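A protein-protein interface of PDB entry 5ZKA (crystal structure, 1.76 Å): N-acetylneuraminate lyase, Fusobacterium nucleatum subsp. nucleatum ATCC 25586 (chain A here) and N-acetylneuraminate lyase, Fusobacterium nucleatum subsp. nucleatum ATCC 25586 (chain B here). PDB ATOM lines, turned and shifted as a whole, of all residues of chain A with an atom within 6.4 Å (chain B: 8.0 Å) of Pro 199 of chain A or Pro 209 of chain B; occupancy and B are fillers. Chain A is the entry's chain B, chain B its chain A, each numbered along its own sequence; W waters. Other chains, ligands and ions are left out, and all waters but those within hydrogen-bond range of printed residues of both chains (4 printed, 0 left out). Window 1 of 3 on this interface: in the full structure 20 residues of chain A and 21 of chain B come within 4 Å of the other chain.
The backbone NH (N) of Tyr 185 of chain B is in hydrogen-bond range of the side-chain sulfur (SD) of Met 196 of chain A (3.4 Å).
The side-chain amide oxygen (OE1) of Gln 239 of chain A lies within hydrogen-bond range of the backbone NH (N) of Leu 198 of chain A (2.9 Å).
The side-chain amide oxygen (OE1) of Gln 249 of chain B lies within hydrogen-bond range of the backbone NH (N) of Leu 208 of chain B, at 2.8 Å.
SD of Met 206 of chain B touches CB of Phe 174 of chain A, at 3.8 Å.
CG of Glu 195 of chain A touches CD1 of Tyr 185 of chain B (3.4 Å).
Phe 184 of chain B touches Met 196 of chain A (CB to SD, 3.8 Å).
Val 212 of chain B touches Leu 198 of chain A.
CB of Pro 199 of chain A touches CB of Pro 209 of chain B (3.7 Å).
Val 202 of chain A touches Leu 208 of chain B (O to CD2, 3.7 Å).
Val 202 of chain A touches Val 212 of chain B (CG2 to CG2, 3.8 Å).
CB of Val 202 of chain A touches CG2 of Ile 242 of chain B, at 3.9 Å.
CD2 of Leu 246 of chain B touches O of Val 202 of chain A, 3.7 Å away.
Leu 203 of chain A touches Leu 246 of chain B.
Pro 199 of chain A touches one residue of chain B.
Pro 209 of chain B touches just one residue of chain A: Pro 199.
Ala 200 of chain A touches none of the printed residues of chain B.
Of the printed residues of chain B, Glu 195 of chain A touches Tyr 185.
Printed residues of chain B within 4 Å of Met 196 of chain A: Phe 184 (3.8 Å) and Tyr 185 (3.4 Å).
Printed residues of chain A within 4 Å of Ile 242 of chain B: Val 202.
Thr 201 of chain A touches none of the printed residues of chain B.
Of the 24 printed residues of chain B, 8 touch a printed residue of chain A.
Printed residues of chain B that touch a printed residue of chain A: Phe 184, Tyr 185, Met 206, Leu 208, Pro 209, Val 212, Ile 242 and Leu 246.
Among the printed residues, 12 pairs touch across the chains.
Among the printed residues, no Asp or Glu carboxylate lies within 4 Å of a Lys or Arg side-chain nitrogen of the other chain.
Water W2 bridges O of Glu 195 of chain A and O of Phe 184 of chain B.
Water W4 bridges O of Glu 205 of chain B (3.0 Å) and O of Phe 174 of chain A (3.0 Å).
Water W3 lies within hydrogen-bond range of N of Phe 174 of chain A and SD of Met 206 of chain B.
Water W1 bridges the backbone NH of Phe 184 of chain B (3.1 Å) and the side-chain sulfur of Met 196 of chain A (3.1 Å).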
ATOM      1  N   PHE A 174      -5.660  -2.831   9.363  1.00  0.00           N
ATOM      2  CA  PHE A 174      -4.287  -2.568   9.790  1.00  0.00           C
ATOM      3  C   PHE A 174      -3.375  -2.121   8.652  1.00  0.00           C
ATOM      4  O   PHE A 174      -2.287  -1.598   8.921  1.00  0.00           O
ATOM      5  CB  PHE A 174      -3.738  -3.804  10.520  1.00  0.00           C
ATOM      6  CG  PHE A 174      -4.306  -3.951  11.902  1.00  0.00           C
ATOM      7  CD1 PHE A 174      -5.584  -4.455  12.084  1.00  0.00           C
ATOM      8  CD2 PHE A 174      -3.597  -3.534  13.008  1.00  0.00           C
ATOM      9  CE1 PHE A 174      -6.139  -4.555  13.345  1.00  0.00           C
ATOM     10  CE2 PHE A 174      -4.152  -3.626  14.287  1.00  0.00           C
ATOM     11  CZ  PHE A 174      -5.430  -4.140  14.447  1.00  0.00           C
ATOM     12  N   LEU A 177      -4.187   1.587   8.865  1.00  0.00           N
ATOM     13  CA  LEU A 177      -3.573   2.107  10.084  1.00  0.00           C
ATOM     14  C   LEU A 177      -2.081   2.362   9.880  1.00  0.00           C
ATOM     15  O   LEU A 177      -1.550   3.394  10.306  1.00  0.00           O
ATOM     16  CB  LEU A 177      -3.806   1.129  11.239  1.00  0.00           C
ATOM     17  CG  LEU A 177      -3.284   1.487  12.630  1.00  0.00           C
ATOM     18  CD1 LEU A 177      -3.981   2.742  13.150  1.00  0.00           C
ATOM     19  CD2 LEU A 177      -3.496   0.318  13.607  1.00  0.00           C
ATOM     20  N   GLU A 195      -9.326  -5.411  21.964  1.00  0.00           N
ATOM     21  CA  GLU A 195      -8.878  -6.773  21.711  1.00  0.00           C
ATOM     22  C   GLU A 195      -7.830  -6.848  20.609  1.00  0.00           C
ATOM     23  O   GLU A 195      -7.394  -7.950  20.258  1.00  0.00           O
ATOM     24  CB  GLU A 195     -10.085  -7.665  21.369  1.00  0.00           C
ATOM     25  CG  GLU A 195     -10.749  -7.408  20.003  1.00  0.00           C
ATOM     26  CD  GLU A 195     -11.535  -6.097  19.917  1.00  0.00           C
ATOM     27  OE1 GLU A 195     -11.678  -5.387  20.939  1.00  0.00           O
ATOM     28  OE2 GLU A 195     -12.013  -5.779  18.804  1.00  0.00           O
ATOM     29  N   MET A 196      -7.421  -5.704  20.051  1.00  0.00           N
ATOM     30  CA  MET A 196      -6.372  -5.665  19.037  1.00  0.00           C
ATOM     31  C   MET A 196      -5.303  -4.642  19.406  1.00  0.00           C
ATOM     32  O   MET A 196      -4.618  -4.095  18.533  1.00  0.00           O
ATOM     33  CB  MET A 196      -6.975  -5.392  17.658  1.00  0.00           C
ATOM     34  CG  MET A 196      -7.923  -6.496  17.239  1.00  0.00           C
ATOM     35  SD  MET A 196      -8.590  -6.389  15.580  1.00  0.00           S
ATOM     36  CE  MET A 196      -9.704  -4.993  15.727  1.00  0.00           C
ATOM     37  N   LEU A 197      -5.101  -4.434  20.708  1.00  0.00           N
ATOM     38  CA  LEU A 197      -4.133  -3.452  21.186  1.00  0.00           C
ATOM     39  C   LEU A 197      -2.703  -3.812  20.775  1.00  0.00           C
ATOM     40  O   LEU A 197      -1.956  -2.956  20.281  1.00  0.00           O
ATOM     41  CB  LEU A 197      -4.255  -3.334  22.704  1.00  0.00           C
ATOM     42  CG  LEU A 197      -3.266  -2.371  23.370  1.00  0.00           C
ATOM     43  CD1 LEU A 197      -3.404  -0.998  22.757  1.00  0.00           C
ATOM     44  CD2 LEU A 197      -3.577  -2.346  24.855  1.00  0.00           C
ATOM     45  N   LEU A 198      -2.306  -5.079  20.946  1.00  0.00           N
ATOM     46  CA  LEU A 198      -0.930  -5.462  20.624  1.00  0.00           C
ATOM     47  C   LEU A 198      -0.577  -5.242  19.158  1.00  0.00           C
ATOM     48  O   LEU A 198       0.451  -4.587  18.894  1.00  0.00           O
ATOM     49  CB  LEU A 198      -0.658  -6.910  21.060  1.00  0.00           C
ATOM     50  CG  LEU A 198       0.670  -7.516  20.560  1.00  0.00           C
ATOM     51  CD1 LEU A 198       1.861  -6.694  20.998  1.00  0.00           C
ATOM     52  CD2 LEU A 198       0.833  -8.942  21.064  1.00  0.00           C
ATOM     53  N   PRO A 199      -1.325  -5.746  18.168  1.00  0.00           N
ATOM     54  CA  PRO A 199      -0.941  -5.450  16.775  1.00  0.00           C
ATOM     55  C   PRO A 199      -0.988  -3.970  16.434  1.00  0.00           C
ATOM     56  O   PRO A 199      -0.208  -3.516  15.579  1.00  0.00           O
ATOM     57  CB  PRO A 199      -1.953  -6.260  15.944  1.00  0.00           C
ATOM     58  CG  PRO A 199      -3.080  -6.554  16.882  1.00  0.00           C
ATOM     59  CD  PRO A 199      -2.449  -6.702  18.221  1.00  0.00           C
ATOM     60  N   ALA A 200      -1.869  -3.198  17.084  1.00  0.00           N
ATOM     61  CA  ALA A 200      -1.876  -1.757  16.857  1.00  0.00           C
ATOM     62  C   ALA A 200      -0.626  -1.101  17.434  1.00  0.00           C
ATOM     63  O   ALA A 200      -0.083  -0.156  16.844  1.00  0.00           O
ATOM     64  CB  ALA A 200      -3.133  -1.132  17.463  1.00  0.00           C
ATOM     65  N   THR A 201      -0.161  -1.580  18.591  1.00  0.00           N
ATOM     66  CA  THR A 201       0.975  -0.942  19.250  1.00  0.00           C
ATOM     67  C   THR A 201       2.238  -1.059  18.403  1.00  0.00           C
ATOM     68  O   THR A 201       3.018  -0.099  18.291  1.00  0.00           O
ATOM     69  CB  THR A 201       1.179  -1.561  20.636  1.00  0.00           C
ATOM     70  OG1 THR A 201       0.003  -1.331  21.418  1.00  0.00           O
ATOM     71  CG2 THR A 201       2.371  -0.930  21.369  1.00  0.00           C
ATOM     72  N   VAL A 202       2.443  -2.214  17.763  1.00  0.00           N
ATOM     73  CA  VAL A 202       3.658  -2.382  16.974  1.00  0.00           C
ATOM     74  C   VAL A 202       3.606  -1.604  15.668  1.00  0.00           C
ATOM     75  O   VAL A 202       4.649  -1.438  15.018  1.00  0.00           O
ATOM     76  CB  VAL A 202       3.967  -3.879  16.730  1.00  0.00           C
ATOM     77  CG1 VAL A 202       3.993  -4.643  18.055  1.00  0.00           C
ATOM     78  CG2 VAL A 202       2.996  -4.515  15.727  1.00  0.00           C
ATOM     79  N   LEU A 203       2.436  -1.099  15.274  1.00  0.00           N
ATOM     80  CA  LEU A 203       2.360  -0.181  14.146  1.00  0.00           C
ATOM     81  C   LEU A 203       2.501   1.270  14.571  1.00  0.00           C
ATOM     82  O   LEU A 203       2.269   2.166  13.749  1.00  0.00           O
ATOM     83  CB  LEU A 203       1.048  -0.357  13.383  1.00  0.00           C
ATOM     84  CG  LEU A 203       0.995  -1.654  12.566  1.00  0.00           C
ATOM     85  CD1 LEU A 203      -0.365  -1.801  11.917  1.00  0.00           C
ATOM     86  CD2 LEU A 203       2.109  -1.656  11.498  1.00  0.00           C
ATOM     87  N   GLY A 204       2.857   1.523  15.831  1.00  0.00           N
ATOM     88  CA  GLY A 204       3.200   2.872  16.262  1.00  0.00           C
ATOM     89  C   GLY A 204       2.053   3.735  16.747  1.00  0.00           C
ATOM     90  O   GLY A 204       2.208   4.967  16.799  1.00  0.00           O
ATOM     91  N   GLN A 239      -2.035 -10.252  26.062  1.00  0.00           N
ATOM     92  CA  GLN A 239      -3.136 -10.030  25.137  1.00  0.00           C
ATOM     93  C   GLN A 239      -4.014 -11.276  25.014  1.00  0.00           C
ATOM     94  O   GLN A 239      -5.245 -11.168  24.913  1.00  0.00           O
ATOM     95  CB  GLN A 239      -2.617  -9.617  23.762  1.00  0.00           C
ATOM     96  CG  GLN A 239      -3.764  -9.310  22.793  1.00  0.00           C
ATOM     97  CD  GLN A 239      -4.339  -7.910  22.993  1.00  0.00           C
ATOM     98  OE1 GLN A 239      -3.650  -6.908  22.772  1.00  0.00           O
ATOM     99  NE2 GLN A 239      -5.604  -7.837  23.398  1.00  0.00           N
ATOM    100  N   PHE B 184      -7.878  -9.221  12.921  1.00  0.00           N
ATOM    101  CA  PHE B 184      -6.798  -9.574  13.833  1.00  0.00           C
ATOM    102  C   PHE B 184      -7.287  -9.983  15.216  1.00  0.00           C
ATOM    103  O   PHE B 184      -6.504 -10.533  15.995  1.00  0.00           O
ATOM    104  CB  PHE B 184      -5.786  -8.411  13.926  1.00  0.00           C
ATOM    105  CG  PHE B 184      -4.880  -8.326  12.738  1.00  0.00           C
ATOM    106  CD1 PHE B 184      -5.362  -7.890  11.514  1.00  0.00           C
ATOM    107  CD2 PHE B 184      -3.552  -8.701  12.835  1.00  0.00           C
ATOM    108  CE1 PHE B 184      -4.527  -7.838  10.398  1.00  0.00           C
ATOM    109  CE2 PHE B 184      -2.713  -8.650  11.726  1.00  0.00           C
ATOM    110  CZ  PHE B 184      -3.202  -8.222  10.511  1.00  0.00           C
ATOM    111  N   TYR B 185      -8.565  -9.776  15.542  1.00  0.00           N
ATOM    112  CA  TYR B 185      -9.103 -10.419  16.731  1.00  0.00           C
ATOM    113  C   TYR B 185      -9.251 -11.919  16.495  1.00  0.00           C
ATOM    114  O   TYR B 185      -8.780 -12.746  17.291  1.00  0.00           O
ATOM    115  CB  TYR B 185     -10.444  -9.775  17.102  1.00  0.00           C
ATOM    116  CG  TYR B 185     -11.159 -10.408  18.281  1.00  0.00           C
ATOM    117  CD1 TYR B 185     -10.473 -10.788  19.432  1.00  0.00           C
ATOM    118  CD2 TYR B 185     -12.529 -10.605  18.243  1.00  0.00           C
ATOM    119  CE1 TYR B 185     -11.144 -11.365  20.521  1.00  0.00           C
ATOM    120  CE2 TYR B 185     -13.217 -11.177  19.327  1.00  0.00           C
ATOM    121  CZ  TYR B 185     -12.518 -11.551  20.461  1.00  0.00           C
ATOM    122  OH  TYR B 185     -13.202 -12.122  21.521  1.00  0.00           O
ATOM    123  N   LEU B 187      -7.625 -13.620  14.358  1.00  0.00           N
ATOM    124  CA  LEU B 187      -6.280 -14.177  14.225  1.00  0.00           C
ATOM    125  C   LEU B 187      -5.699 -14.515  15.589  1.00  0.00           C
ATOM    126  O   LEU B 187      -5.135 -15.595  15.782  1.00  0.00           O
ATOM    127  CB  LEU B 187      -5.364 -13.204  13.469  1.00  0.00           C
ATOM    128  CG  LEU B 187      -3.886 -13.618  13.337  1.00  0.00           C
ATOM    129  CD1 LEU B 187      -3.739 -15.013  12.710  1.00  0.00           C
ATOM    130  CD2 LEU B 187      -3.068 -12.568  12.568  1.00  0.00           C
ATOM    131  N   GLU B 188      -5.852 -13.612  16.560  1.00  0.00           N
ATOM    132  CA  GLU B 188      -5.359 -13.891  17.903  1.00  0.00           C
ATOM    133  C   GLU B 188      -6.120 -15.046  18.553  1.00  0.00           C
ATOM    134  O   GLU B 188      -5.528 -15.854  19.280  1.00  0.00           O
ATOM    135  CB  GLU B 188      -5.449 -12.612  18.754  1.00  0.00           C
ATOM    136  CG  GLU B 188      -5.024 -12.775  20.224  1.00  0.00           C
ATOM    137  CD  GLU B 188      -6.109 -13.417  21.094  1.00  0.00           C
ATOM    138  OE1 GLU B 188      -7.302 -13.164  20.824  1.00  0.00           O
ATOM    139  OE2 GLU B 188      -5.768 -14.180  22.022  1.00  0.00           O
ATOM    140  N   ALA B 201       0.286 -15.962   7.542  1.00  0.00           N
ATOM    141  CA  ALA B 201      -0.352 -14.715   7.147  1.00  0.00           C
ATOM    142  C   ALA B 201      -0.461 -14.632   5.631  1.00  0.00           C
ATOM    143  O   ALA B 201       0.506 -14.913   4.921  1.00  0.00           O
ATOM    144  CB  ALA B 201       0.444 -13.520   7.681  1.00  0.00           C
ATOM    145  N   PHE B 203      -1.627 -11.689   4.044  1.00  0.00           N
ATOM    146  CA  PHE B 203      -1.750 -10.265   3.724  1.00  0.00           C
ATOM    147  C   PHE B 203      -0.377  -9.616   3.901  1.00  0.00           C
ATOM    148  O   PHE B 203       0.003  -9.259   5.021  1.00  0.00           O
ATOM    149  CB  PHE B 203      -2.812  -9.637   4.629  1.00  0.00           C
ATOM    150  CG  PHE B 203      -2.890 -10.292   6.000  1.00  0.00           C
ATOM    151  CD1 PHE B 203      -1.785 -10.310   6.836  1.00  0.00           C
ATOM    152  CD2 PHE B 203      -4.053 -10.909   6.437  1.00  0.00           C
ATOM    153  CE1 PHE B 203      -1.831 -10.912   8.073  1.00  0.00           C
ATOM    154  CE2 PHE B 203      -4.103 -11.516   7.687  1.00  0.00           C
ATOM    155  CZ  PHE B 203      -2.988 -11.514   8.501  1.00  0.00           C
ATOM    156  N   ASP B 204       0.372  -9.467   2.792  1.00  0.00           N
ATOM    157  CA  ASP B 204       1.766  -9.045   2.864  1.00  0.00           C
ATOM    158  C   ASP B 204       1.900  -7.681   3.507  1.00  0.00           C
ATOM    159  O   ASP B 204       2.914  -7.390   4.153  1.00  0.00           O
ATOM    160  CB  ASP B 204       2.375  -8.958   1.467  1.00  0.00           C
ATOM    161  CG  ASP B 204       2.296 -10.265   0.696  1.00  0.00           C
ATOM    162  OD1 ASP B 204       1.527 -11.154   1.109  1.00  0.00           O
ATOM    163  OD2 ASP B 204       3.000 -10.376  -0.335  1.00  0.00           O
ATOM    164  N   GLU B 205       0.905  -6.822   3.305  1.00  0.00           N
ATOM    165  CA  GLU B 205       0.968  -5.462   3.814  1.00  0.00           C
ATOM    166  C   GLU B 205       0.658  -5.387   5.302  1.00  0.00           C
ATOM    167  O   GLU B 205       0.702  -4.293   5.869  1.00  0.00           O
ATOM    168  CB  GLU B 205       0.008  -4.562   3.023  1.00  0.00           C
ATOM    169  CG  GLU B 205      -1.476  -4.831   3.230  1.00  0.00           C
ATOM    170  CD  GLU B 205      -2.007  -6.002   2.418  1.00  0.00           C
ATOM    171  OE1 GLU B 205      -1.228  -6.649   1.674  1.00  0.00           O
ATOM    172  OE2 GLU B 205      -3.225  -6.250   2.513  1.00  0.00           O
ATOM    173  N   MET B 206       0.326  -6.515   5.935  1.00  0.00           N
ATOM    174  CA  MET B 206       0.090  -6.586   7.374  1.00  0.00           C
ATOM    175  C   MET B 206       0.956  -7.665   8.025  1.00  0.00           C
ATOM    176  O   MET B 206       0.570  -8.263   9.030  1.00  0.00           O
ATOM    177  CB  MET B 206      -1.389  -6.812   7.656  1.00  0.00           C
ATOM    178  CG  MET B 206      -2.240  -5.774   6.926  1.00  0.00           C
ATOM    179  SD  MET B 206      -3.993  -5.817   7.354  1.00  0.00           S
ATOM    180  CE  MET B 206      -4.465  -7.398   6.678  1.00  0.00           C
ATOM    181  N   LEU B 207       2.155  -7.890   7.475  1.00  0.00           N
ATOM    182  CA  LEU B 207       3.032  -8.939   7.986  1.00  0.00           C
ATOM    183  C   LEU B 207       3.495  -8.644   9.408  1.00  0.00           C
ATOM    184  O   LEU B 207       3.536  -9.542  10.255  1.00  0.00           O
ATOM    185  CB  LEU B 207       4.239  -9.096   7.056  1.00  0.00           C
ATOM    186  CG  LEU B 207       5.290 -10.140   7.449  1.00  0.00           C
ATOM    187  CD1 LEU B 207       4.656 -11.527   7.633  1.00  0.00           C
ATOM    188  CD2 LEU B 207       6.368 -10.205   6.369  1.00  0.00           C
ATOM    189  N   LEU B 208       3.838  -7.392   9.696  1.00  0.00           N
ATOM    190  CA  LEU B 208       4.358  -7.083  11.029  1.00  0.00           C
ATOM    191  C   LEU B 208       3.309  -7.300  12.116  1.00  0.00           C
ATOM    192  O   LEU B 208       3.608  -8.009  13.096  1.00  0.00           O
ATOM    193  CB  LEU B 208       4.931  -5.662  11.048  1.00  0.00           C
ATOM    194  CG  LEU B 208       5.203  -5.059  12.426  1.00  0.00           C
ATOM    195  CD1 LEU B 208       6.183  -5.895  13.233  1.00  0.00           C
ATOM    196  CD2 LEU B 208       5.745  -3.646  12.235  1.00  0.00           C
ATOM    197  N   PRO B 209       2.093  -6.748  12.031  1.00  0.00           N
ATOM    198  CA  PRO B 209       1.118  -7.019  13.105  1.00  0.00           C
ATOM    199  C   PRO B 209       0.769  -8.493  13.236  1.00  0.00           C
ATOM    200  O   PRO B 209       0.543  -8.981  14.350  1.00  0.00           O
ATOM    201  CB  PRO B 209      -0.105  -6.177  12.707  1.00  0.00           C
ATOM    202  CG  PRO B 209       0.106  -5.803  11.266  1.00  0.00           C
ATOM    203  CD  PRO B 209       1.595  -5.738  11.076  1.00  0.00           C
ATOM    204  N   ALA B 210       0.747  -9.229  12.125  1.00  0.00           N
ATOM    205  CA  ALA B 210       0.515 -10.669  12.197  1.00  0.00           C
ATOM    206  C   ALA B 210       1.661 -11.387  12.899  1.00  0.00           C
ATOM    207  O   ALA B 210       1.433 -12.319  13.676  1.00  0.00           O
ATOM    208  CB  ALA B 210       0.325 -11.229  10.786  1.00  0.00           C
ATOM    209  N   THR B 211       2.909 -10.978  12.627  1.00  0.00           N
ATOM    210  CA  THR B 211       4.048 -11.656  13.241  1.00  0.00           C
ATOM    211  C   THR B 211       3.996 -11.582  14.766  1.00  0.00           C
ATOM    212  O   THR B 211       4.298 -12.568  15.451  1.00  0.00           O
ATOM    213  CB  THR B 211       5.357 -11.061  12.711  1.00  0.00           C
ATOM    214  OG1 THR B 211       5.377 -11.222  11.288  1.00  0.00           O
ATOM    215  CG2 THR B 211       6.552 -11.798  13.299  1.00  0.00           C
ATOM    216  N   VAL B 212       3.607 -10.435  15.329  1.00  0.00           N
ATOM    217  CA  VAL B 212       3.622 -10.349  16.789  1.00  0.00           C
ATOM    218  C   VAL B 212       2.432 -11.053  17.433  1.00  0.00           C
ATOM    219  O   VAL B 212       2.430 -11.243  18.659  1.00  0.00           O
ATOM    220  CB  VAL B 212       3.704  -8.883  17.263  1.00  0.00           C
ATOM    221  CG1 VAL B 212       4.937  -8.190  16.640  1.00  0.00           C
ATOM    222  CG2 VAL B 212       2.411  -8.114  16.957  1.00  0.00           C
ATOM    223  N   LEU B 213       1.423 -11.447  16.653  1.00  0.00           N
ATOM    224  CA  LEU B 213       0.382 -12.361  17.119  1.00  0.00           C
ATOM    225  C   LEU B 213       0.776 -13.827  16.950  1.00  0.00           C
ATOM    226  O   LEU B 213      -0.061 -14.710  17.144  1.00  0.00           O
ATOM    227  CB  LEU B 213      -0.935 -12.105  16.375  1.00  0.00           C
ATOM    228  CG  LEU B 213      -1.651 -10.796  16.743  1.00  0.00           C
ATOM    229  CD1 LEU B 213      -2.945 -10.663  15.958  1.00  0.00           C
ATOM    230  CD2 LEU B 213      -1.961 -10.748  18.243  1.00  0.00           C
ATOM    231  N   GLY B 214       2.026 -14.102  16.571  1.00  0.00           N
ATOM    232  CA  GLY B 214       2.554 -15.452  16.614  1.00  0.00           C
ATOM    233  C   GLY B 214       2.316 -16.315  15.393  1.00  0.00           C
ATOM    234  O   GLY B 214       2.399 -17.545  15.511  1.00  0.00           O
ATOM    235  N   VAL B 215       2.047 -15.731  14.220  1.00  0.00           N
ATOM    236  CA  VAL B 215       1.943 -16.580  13.023  1.00  0.00           C
ATOM    237  C   VAL B 215       3.291 -17.274  12.771  1.00  0.00           C
ATOM    238  O   VAL B 215       4.351 -16.828  13.224  1.00  0.00           O
ATOM    239  CB  VAL B 215       1.491 -15.811  11.769  1.00  0.00           C
ATOM    240  CG1 VAL B 215       0.094 -15.240  11.947  1.00  0.00           C
ATOM    241  CG2 VAL B 215       2.483 -14.715  11.420  1.00  0.00           C
ATOM    242  N   ILE B 233      11.338  -8.225   8.108  1.00  0.00           N
ATOM    243  CA  ILE B 233      10.220  -7.882   8.999  1.00  0.00           C
ATOM    244  C   ILE B 233       9.924  -9.042   9.941  1.00  0.00           C
ATOM    245  O   ILE B 233       9.889  -8.883  11.169  1.00  0.00           O
ATOM    246  CB  ILE B 233       8.969  -7.499   8.190  1.00  0.00           C
ATOM    247  CG1 ILE B 233       9.193  -6.223   7.364  1.00  0.00           C
ATOM    248  CG2 ILE B 233       7.751  -7.354   9.131  1.00  0.00           C
ATOM    249  CD1 ILE B 233       8.121  -6.001   6.265  1.00  0.00           C
ATOM    250  N   ALA B 237      10.817  -8.828  13.955  1.00  0.00           N
ATOM    251  CA  ALA B 237       9.691  -8.726  14.881  1.00  0.00           C
ATOM    252  C   ALA B 237       9.687  -9.857  15.904  1.00  0.00           C
ATOM    253  O   ALA B 237       9.200  -9.668  17.026  1.00  0.00           O
ATOM    254  CB  ALA B 237       8.360  -8.699  14.116  1.00  0.00           C
ATOM    255  N   ILE B 242      11.414  -4.342  17.043  1.00  0.00           N
ATOM    256  CA  ILE B 242      10.138  -3.903  16.474  1.00  0.00           C
ATOM    257  C   ILE B 242      10.304  -2.590  15.721  1.00  0.00           C
ATOM    258  O   ILE B 242       9.731  -2.401  14.640  1.00  0.00           O
ATOM    259  CB  ILE B 242       9.074  -3.783  17.577  1.00  0.00           C
ATOM    260  CG1 ILE B 242       8.784  -5.147  18.175  1.00  0.00           C
ATOM    261  CG2 ILE B 242       7.791  -3.186  17.011  1.00  0.00           C
ATOM    262  CD1 ILE B 242       8.056  -6.042  17.226  1.00  0.00           C
ATOM    263  N   LEU B 246       9.202  -2.079  11.857  1.00  0.00           N
ATOM    264  CA  LEU B 246       8.184  -1.133  11.407  1.00  0.00           C
ATOM    265  C   LEU B 246       8.695  -0.266  10.270  1.00  0.00           C
ATOM    266  O   LEU B 246       7.948   0.029   9.328  1.00  0.00           O
ATOM    267  CB  LEU B 246       7.717  -0.258  12.576  1.00  0.00           C
ATOM    268  CG  LEU B 246       6.644   0.791  12.278  1.00  0.00           C
ATOM    269  CD1 LEU B 246       5.427   0.136  11.647  1.00  0.00           C
ATOM    270  CD2 LEU B 246       6.219   1.550  13.553  1.00  0.00           C
ATOM    271  N   GLN B 249       8.485  -2.426   7.254  1.00  0.00           N
ATOM    272  CA  GLN B 249       7.089  -2.565   6.828  1.00  0.00           C
ATOM    273  C   GLN B 249       6.591  -1.289   6.159  1.00  0.00           C
ATOM    274  O   GLN B 249       5.822  -1.345   5.188  1.00  0.00           O
ATOM    275  CB  GLN B 249       6.194  -2.919   8.014  1.00  0.00           C
ATOM    276  CG  GLN B 249       4.737  -3.194   7.634  1.00  0.00           C
ATOM    277  CD  GLN B 249       4.578  -4.577   7.037  1.00  0.00           C
ATOM    278  OE1 GLN B 249       4.715  -5.569   7.747  1.00  0.00           O
ATOM    279  NE2 GLN B 249       4.319  -4.652   5.731  1.00  0.00           N
ATOM    280  N   ASN B 253       5.287  -1.180   2.389  1.00  0.00           N
ATOM    281  CA  ASN B 253       3.934  -0.781   2.029  1.00  0.00           C
ATOM    282  C   ASN B 253       3.892   0.421   1.089  1.00  0.00           C
ATOM    283  O   ASN B 253       2.892   0.601   0.391  1.00  0.00           O
ATOM    284  CB  ASN B 253       3.108  -0.537   3.304  1.00  0.00           C
ATOM    285  CG  ASN B 253       2.697  -1.843   3.970  1.00  0.00           C
ATOM    286  OD1 ASN B 253       3.149  -2.913   3.559  1.00  0.00           O
ATOM    287  ND2 ASN B 253       1.836  -1.770   4.988  1.00  0.00           N
HETATM  288  O   HOH W   1      -9.037  -6.393  12.475  1.00  0.00           O
HETATM  289  O   HOH W   2      -5.440  -9.033  18.409  1.00  0.00           O
HETATM  290  O   HOH W   3      -6.930  -5.457   8.820  1.00  0.00           O
HETATM  291  O   HOH W   4       0.152  -3.290   8.594  1.00  0.00           O
